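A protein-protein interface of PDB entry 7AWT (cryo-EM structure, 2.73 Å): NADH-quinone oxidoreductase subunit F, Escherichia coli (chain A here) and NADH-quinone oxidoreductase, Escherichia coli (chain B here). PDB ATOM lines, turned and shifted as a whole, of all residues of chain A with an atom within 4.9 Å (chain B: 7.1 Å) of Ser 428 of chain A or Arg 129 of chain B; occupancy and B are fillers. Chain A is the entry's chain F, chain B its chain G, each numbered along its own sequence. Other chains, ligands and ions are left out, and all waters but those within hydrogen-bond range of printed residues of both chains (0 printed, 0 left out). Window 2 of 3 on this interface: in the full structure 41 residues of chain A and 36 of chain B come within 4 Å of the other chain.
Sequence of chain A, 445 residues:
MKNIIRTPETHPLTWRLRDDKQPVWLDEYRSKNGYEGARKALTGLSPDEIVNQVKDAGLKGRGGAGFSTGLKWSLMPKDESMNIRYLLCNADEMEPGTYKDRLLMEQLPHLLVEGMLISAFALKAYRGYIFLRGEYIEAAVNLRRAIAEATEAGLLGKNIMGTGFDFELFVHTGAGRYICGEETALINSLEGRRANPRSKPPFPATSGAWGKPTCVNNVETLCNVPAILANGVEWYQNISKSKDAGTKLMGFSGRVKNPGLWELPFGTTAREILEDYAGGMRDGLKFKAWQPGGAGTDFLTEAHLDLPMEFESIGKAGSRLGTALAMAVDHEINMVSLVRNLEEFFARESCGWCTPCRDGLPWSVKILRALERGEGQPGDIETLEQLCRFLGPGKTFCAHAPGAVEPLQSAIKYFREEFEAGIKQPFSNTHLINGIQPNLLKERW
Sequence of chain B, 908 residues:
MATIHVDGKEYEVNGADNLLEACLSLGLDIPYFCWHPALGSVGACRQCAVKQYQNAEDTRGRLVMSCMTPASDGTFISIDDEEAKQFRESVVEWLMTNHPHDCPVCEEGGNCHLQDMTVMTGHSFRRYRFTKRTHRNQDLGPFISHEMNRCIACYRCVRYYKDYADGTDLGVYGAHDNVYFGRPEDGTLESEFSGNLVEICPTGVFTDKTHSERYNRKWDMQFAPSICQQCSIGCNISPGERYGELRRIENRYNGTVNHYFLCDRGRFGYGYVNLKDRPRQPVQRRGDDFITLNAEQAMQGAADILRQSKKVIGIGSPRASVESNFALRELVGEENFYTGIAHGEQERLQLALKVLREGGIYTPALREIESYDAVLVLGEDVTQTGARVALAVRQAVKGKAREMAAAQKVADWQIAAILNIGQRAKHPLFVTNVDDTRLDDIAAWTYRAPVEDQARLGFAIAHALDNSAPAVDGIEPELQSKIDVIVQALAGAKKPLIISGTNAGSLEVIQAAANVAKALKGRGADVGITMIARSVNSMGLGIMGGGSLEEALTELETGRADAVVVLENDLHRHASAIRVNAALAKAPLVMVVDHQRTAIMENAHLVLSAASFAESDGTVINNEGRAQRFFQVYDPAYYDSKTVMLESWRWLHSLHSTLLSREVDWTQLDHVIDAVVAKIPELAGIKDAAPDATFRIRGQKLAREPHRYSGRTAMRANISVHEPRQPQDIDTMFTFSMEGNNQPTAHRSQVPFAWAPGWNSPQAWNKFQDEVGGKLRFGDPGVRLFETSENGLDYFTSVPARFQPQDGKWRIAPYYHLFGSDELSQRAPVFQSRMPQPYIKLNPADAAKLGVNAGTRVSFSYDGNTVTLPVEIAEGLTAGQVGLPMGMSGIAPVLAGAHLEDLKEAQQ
The side-chain amide oxygen (OE1) of Gln 377 of chain A lies within hydrogen-bond range of the guanidinium group (NH2) of Arg 129 of chain B (3.0 Å).
OD2 of Asp 380 of chain A is in salt-bridge range of NH1 of Arg 129 of chain B (3.6 Å).
O of Arg 126 of chain B lies within hydrogen-bond range of ND2 of Asn 429 of chain A (3.1 Å).
The backbone carbonyl oxygen (O) of Tyr 128 of chain B is in hydrogen-bond range of the side-chain amide nitrogen (ND2) of Asn 429 of chain A, 2.9 Å away.
N of Gln 377 of chain A lies within hydrogen-bond range of OD2 of Asp 380 of chain A.
O of Thr 97 of chain B lies within hydrogen-bond range of NH1 of Arg 126 of chain B, 3.0 Å away.
The side-chain hydroxyl (OH) of Tyr 128 of chain B is in hydrogen-bond range of the backbone carbonyl oxygen (O) of Thr 131 of chain B (3.3 Å).
Among the printed residues, pairs that only touch across the chains: Ser 428 of chain A with Arg 129 of chain B.
Ala 370 of chain A touches none of the printed residues of chain B.
Of the printed residues of chain B, Asp 380 of chain A touches Arg 129 (3.6 Å).
Ser 428 of chain A touches just one residue of chain B: Arg 129 (3.9 Å).
Printed residues of chain B within 4 Å of Asn 429 of chain A: Arg 126 and Tyr 128.
Of the printed residues of chain A, Tyr 128 of chain B touches Asn 429 (2.9 Å).
Of chain A, only Gln 377, Asp 380 and Ser 428 come within 4 Å of Arg 129 of chain B.
Along chain B the printed residues that touch a printed residue of chain A span positions 126 to 129.
Among the printed residues, Asp or Glu carboxylates within 4 Å of a Lys or Arg side-chain nitrogen of the other chain: Asp 380 of chain A with Arg 129 of chain B (3.6 Å).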
ATOM      1  N   ALA A 370       3.261 -16.851  -2.998  1.00  0.00           N
ATOM      2  CA  ALA A 370       3.060 -18.051  -3.801  1.00  0.00           C
ATOM      3  C   ALA A 370       2.102 -17.792  -4.956  1.00  0.00           C
ATOM      4  O   ALA A 370       2.265 -18.359  -6.042  1.00  0.00           O
ATOM      5  CB  ALA A 370       2.543 -19.187  -2.923  1.00  0.00           C
ATOM      6  N   GLU A 375       2.611 -20.366  -7.843  1.00  0.00           N
ATOM      7  CA  GLU A 375       2.570 -21.611  -7.088  1.00  0.00           C
ATOM      8  C   GLU A 375       1.417 -21.612  -6.095  1.00  0.00           C
ATOM      9  O   GLU A 375       1.537 -22.115  -4.978  1.00  0.00           O
ATOM     10  CB  GLU A 375       3.888 -21.862  -6.363  1.00  0.00           C
ATOM     11  CG  GLU A 375       5.128 -21.474  -7.139  1.00  0.00           C
ATOM     12  CD  GLU A 375       6.322 -21.251  -6.235  1.00  0.00           C
ATOM     13  OE1 GLU A 375       6.636 -20.082  -5.939  1.00  0.00           O
ATOM     14  OE2 GLU A 375       6.944 -22.249  -5.817  1.00  0.00           O
ATOM     15  N   GLN A 377      -2.400 -22.777  -4.779  1.00  0.00           N
ATOM     16  CA  GLN A 377      -3.033 -24.079  -4.680  1.00  0.00           C
ATOM     17  C   GLN A 377      -4.485 -23.906  -4.267  1.00  0.00           C
ATOM     18  O   GLN A 377      -4.835 -22.898  -3.641  1.00  0.00           O
ATOM     19  CB  GLN A 377      -2.307 -24.977  -3.667  1.00  0.00           C
ATOM     20  CG  GLN A 377      -0.955 -25.446  -4.150  1.00  0.00           C
ATOM     21  CD  GLN A 377      -0.174 -26.154  -3.080  1.00  0.00           C
ATOM     22  OE1 GLN A 377      -0.607 -26.245  -1.934  1.00  0.00           O
ATOM     23  NE2 GLN A 377       0.998 -26.656  -3.443  1.00  0.00           N
ATOM     24  N   ASP A 380      -6.423 -21.502  -1.350  1.00  0.00           N
ATOM     25  CA  ASP A 380      -5.618 -20.344  -0.981  1.00  0.00           C
ATOM     26  C   ASP A 380      -6.485 -19.101  -0.833  1.00  0.00           C
ATOM     27  O   ASP A 380      -6.474 -18.443   0.211  1.00  0.00           O
ATOM     28  CB  ASP A 380      -4.520 -20.114  -2.018  1.00  0.00           C
ATOM     29  CG  ASP A 380      -3.242 -20.853  -1.687  1.00  0.00           C
ATOM     30  OD1 ASP A 380      -3.140 -21.396  -0.568  1.00  0.00           O
ATOM     31  OD2 ASP A 380      -2.335 -20.895  -2.545  1.00  0.00           O
ATOM     32  N   PRO A 426      -1.794 -28.337  -7.514  1.00  0.00           N
ATOM     33  CA  PRO A 426      -2.716 -29.271  -6.892  1.00  0.00           C
ATOM     34  C   PRO A 426      -2.400 -29.196  -5.429  1.00  0.00           C
ATOM     35  O   PRO A 426      -1.224 -29.203  -5.098  1.00  0.00           O
ATOM     36  CB  PRO A 426      -2.272 -30.596  -7.467  1.00  0.00           C
ATOM     37  CG  PRO A 426      -0.812 -30.431  -7.650  1.00  0.00           C
ATOM     38  CD  PRO A 426      -0.531 -28.983  -7.875  1.00  0.00           C
ATOM     39  N   PHE A 427      -3.389 -29.119  -4.556  1.00  0.00           N
ATOM     40  CA  PHE A 427      -3.017 -28.975  -3.176  1.00  0.00           C
ATOM     41  C   PHE A 427      -2.342 -30.192  -2.691  1.00  0.00           C
ATOM     42  O   PHE A 427      -2.874 -31.274  -2.803  1.00  0.00           O
ATOM     43  CB  PHE A 427      -4.221 -28.799  -2.283  1.00  0.00           C
ATOM     44  CG  PHE A 427      -3.860 -28.666  -0.841  1.00  0.00           C
ATOM     45  CD1 PHE A 427      -3.171 -27.556  -0.397  1.00  0.00           C
ATOM     46  CD2 PHE A 427      -4.192 -29.644   0.059  1.00  0.00           C
ATOM     47  CE1 PHE A 427      -2.820 -27.417   0.926  1.00  0.00           C
ATOM     48  CE2 PHE A 427      -3.855 -29.514   1.387  1.00  0.00           C
ATOM     49  CZ  PHE A 427      -3.164 -28.403   1.819  1.00  0.00           C
ATOM     50  N   SER A 428      -1.159 -30.016  -2.146  1.00  0.00           N
ATOM     51  CA  SER A 428      -0.474 -31.130  -1.552  1.00  0.00           C
ATOM     52  C   SER A 428       0.341 -30.569  -0.436  1.00  0.00           C
ATOM     53  O   SER A 428       0.997 -29.559  -0.572  1.00  0.00           O
ATOM     54  CB  SER A 428       0.382 -31.900  -2.541  1.00  0.00           C
ATOM     55  OG  SER A 428       1.061 -32.954  -1.874  1.00  0.00           O
ATOM     56  N   ASN A 429       0.326 -31.278   0.665  1.00  0.00           N
ATOM     57  CA  ASN A 429       1.040 -30.842   1.820  1.00  0.00           C
ATOM     58  C   ASN A 429       1.892 -31.945   2.447  1.00  0.00           C
ATOM     59  O   ASN A 429       2.843 -31.648   3.130  1.00  0.00           O
ATOM     60  CB  ASN A 429       0.010 -30.382   2.798  1.00  0.00           C
ATOM     61  CG  ASN A 429       0.599 -29.616   3.892  1.00  0.00           C
ATOM     62  OD1 ASN A 429       1.792 -29.487   3.978  1.00  0.00           O
ATOM     63  ND2 ASN A 429      -0.228 -29.095   4.741  1.00  0.00           N
ATOM     64  N   THR A 430       1.575 -33.216   2.203  1.00  0.00           N
ATOM     65  CA  THR A 430       2.363 -34.289   2.786  1.00  0.00           C
ATOM     66  C   THR A 430       3.553 -34.612   1.882  1.00  0.00           C
ATOM     67  O   THR A 430       3.752 -34.000   0.830  1.00  0.00           O
ATOM     68  CB  THR A 430       1.493 -35.523   3.012  1.00  0.00           C
ATOM     69  OG1 THR A 430       0.984 -35.985   1.756  1.00  0.00           O
ATOM     70  CG2 THR A 430       0.330 -35.189   3.927  1.00  0.00           C
ATOM     71  N   THR B  97       1.067 -22.894  13.102  1.00  0.00           N
ATOM     72  CA  THR B  97       1.771 -22.623  11.852  1.00  0.00           C
ATOM     73  C   THR B  97       3.281 -22.678  12.040  1.00  0.00           C
ATOM     74  O   THR B  97       4.003 -23.181  11.174  1.00  0.00           O
ATOM     75  CB  THR B  97       1.364 -21.263  11.290  1.00  0.00           C
ATOM     76  OG1 THR B  97       1.511 -20.263  12.301  1.00  0.00           O
ATOM     77  CG2 THR B  97      -0.067 -21.286  10.815  1.00  0.00           C
ATOM     78  N   ARG B 126      -3.554 -29.901   9.276  1.00  0.00           N
ATOM     79  CA  ARG B 126      -2.638 -28.822   8.935  1.00  0.00           C
ATOM     80  C   ARG B 126      -2.900 -28.347   7.513  1.00  0.00           C
ATOM     81  O   ARG B 126      -2.730 -29.111   6.557  1.00  0.00           O
ATOM     82  CB  ARG B 126      -1.188 -29.273   9.081  1.00  0.00           C
ATOM     83  CG  ARG B 126      -0.191 -28.139   9.006  1.00  0.00           C
ATOM     84  CD  ARG B 126       1.222 -28.638   9.184  1.00  0.00           C
ATOM     85  NE  ARG B 126       2.191 -27.555   9.092  1.00  0.00           N
ATOM     86  CZ  ARG B 126       2.531 -26.777  10.110  1.00  0.00           C
ATOM     87  NH1 ARG B 126       3.423 -25.814   9.940  1.00  0.00           N
ATOM     88  NH2 ARG B 126       1.978 -26.961  11.296  1.00  0.00           N
ATOM     89  N   ARG B 127      -3.306 -27.087   7.377  1.00  0.00           N
ATOM     90  CA  ARG B 127      -3.403 -26.446   6.076  1.00  0.00           C
ATOM     91  C   ARG B 127      -2.177 -25.618   5.735  1.00  0.00           C
ATOM     92  O   ARG B 127      -1.952 -25.331   4.555  1.00  0.00           O
ATOM     93  CB  ARG B 127      -4.640 -25.547   6.010  1.00  0.00           C
ATOM     94  CG  ARG B 127      -5.951 -26.282   6.142  1.00  0.00           C
ATOM     95  CD  ARG B 127      -7.109 -25.321   5.999  1.00  0.00           C
ATOM     96  NE  ARG B 127      -7.035 -24.240   6.973  1.00  0.00           N
ATOM     97  CZ  ARG B 127      -7.745 -23.122   6.898  1.00  0.00           C
ATOM     98  NH1 ARG B 127      -8.584 -22.936   5.890  1.00  0.00           N
ATOM     99  NH2 ARG B 127      -7.617 -22.190   7.830  1.00  0.00           N
ATOM    100  N   TYR B 128      -1.399 -25.218   6.736  1.00  0.00           N
ATOM    101  CA  TYR B 128      -0.157 -24.508   6.485  1.00  0.00           C
ATOM    102  C   TYR B 128       0.775 -25.364   5.638  1.00  0.00           C
ATOM    103  O   TYR B 128       0.780 -26.593   5.725  1.00  0.00           O
ATOM    104  CB  TYR B 128       0.515 -24.141   7.804  1.00  0.00           C
ATOM    105  CG  TYR B 128       1.499 -23.005   7.707  1.00  0.00           C
ATOM    106  CD1 TYR B 128       1.082 -21.729   7.378  1.00  0.00           C
ATOM    107  CD2 TYR B 128       2.843 -23.204   7.962  1.00  0.00           C
ATOM    108  CE1 TYR B 128       1.976 -20.688   7.295  1.00  0.00           C
ATOM    109  CE2 TYR B 128       3.742 -22.168   7.881  1.00  0.00           C
ATOM    110  CZ  TYR B 128       3.303 -20.913   7.550  1.00  0.00           C
ATOM    111  OH  TYR B 128       4.197 -19.876   7.468  1.00  0.00           O
ATOM    112  N   ARG B 129       1.564 -24.699   4.807  1.00  0.00           N
ATOM    113  CA  ARG B 129       2.403 -25.370   3.828  1.00  0.00           C
ATOM    114  C   ARG B 129       3.835 -24.866   3.801  1.00  0.00           C
ATOM    115  O   ARG B 129       4.726 -25.619   3.391  1.00  0.00           O
ATOM    116  CB  ARG B 129       1.785 -25.213   2.430  1.00  0.00           C
ATOM    117  CG  ARG B 129       2.599 -25.750   1.284  1.00  0.00           C
ATOM    118  CD  ARG B 129       1.776 -25.776   0.017  1.00  0.00           C
ATOM    119  NE  ARG B 129       1.644 -24.459  -0.594  1.00  0.00           N
ATOM    120  CZ  ARG B 129       0.566 -23.690  -0.487  1.00  0.00           C
ATOM    121  NH1 ARG B 129       0.529 -22.506  -1.081  1.00  0.00           N
ATOM    122  NH2 ARG B 129      -0.474 -24.106   0.218  1.00  0.00           N
ATOM    123  N   PHE B 130       4.022 -23.629   4.220  1.00  0.00           N
ATOM    124  CA  PHE B 130       5.271 -22.882   4.221  1.00  0.00           C
ATOM    125  C   PHE B 130       6.215 -23.131   5.380  1.00  0.00           C
ATOM    126  O   PHE B 130       5.909 -23.901   6.267  1.00  0.00           O
ATOM    127  CB  PHE B 130       4.919 -21.421   4.053  1.00  0.00           C
ATOM    128  CG  PHE B 130       3.767 -21.221   3.130  1.00  0.00           C
ATOM    129  CD1 PHE B 130       3.922 -21.408   1.790  1.00  0.00           C
ATOM    130  CD2 PHE B 130       2.534 -20.909   3.609  1.00  0.00           C
ATOM    131  CE1 PHE B 130       2.871 -21.257   0.934  1.00  0.00           C
ATOM    132  CE2 PHE B 130       1.480 -20.762   2.766  1.00  0.00           C
ATOM    133  CZ  PHE B 130       1.647 -20.935   1.425  1.00  0.00           C
ATOM    134  N   THR B 131       7.387 -22.509   5.343  1.00  0.00           N
ATOM    135  CA  THR B 131       8.404 -22.730   6.352  1.00  0.00           C
ATOM    136  C   THR B 131       7.969 -22.176   7.704  1.00  0.00           C
ATOM    137  O   THR B 131       7.099 -21.309   7.801  1.00  0.00           O
ATOM    138  CB  THR B 131       9.719 -22.082   5.929  1.00  0.00           C
ATOM    139  OG1 THR B 131       9.483 -20.709   5.594  1.00  0.00           O
ATOM    140  CG2 THR B 131      10.292 -22.791   4.718  1.00  0.00           C
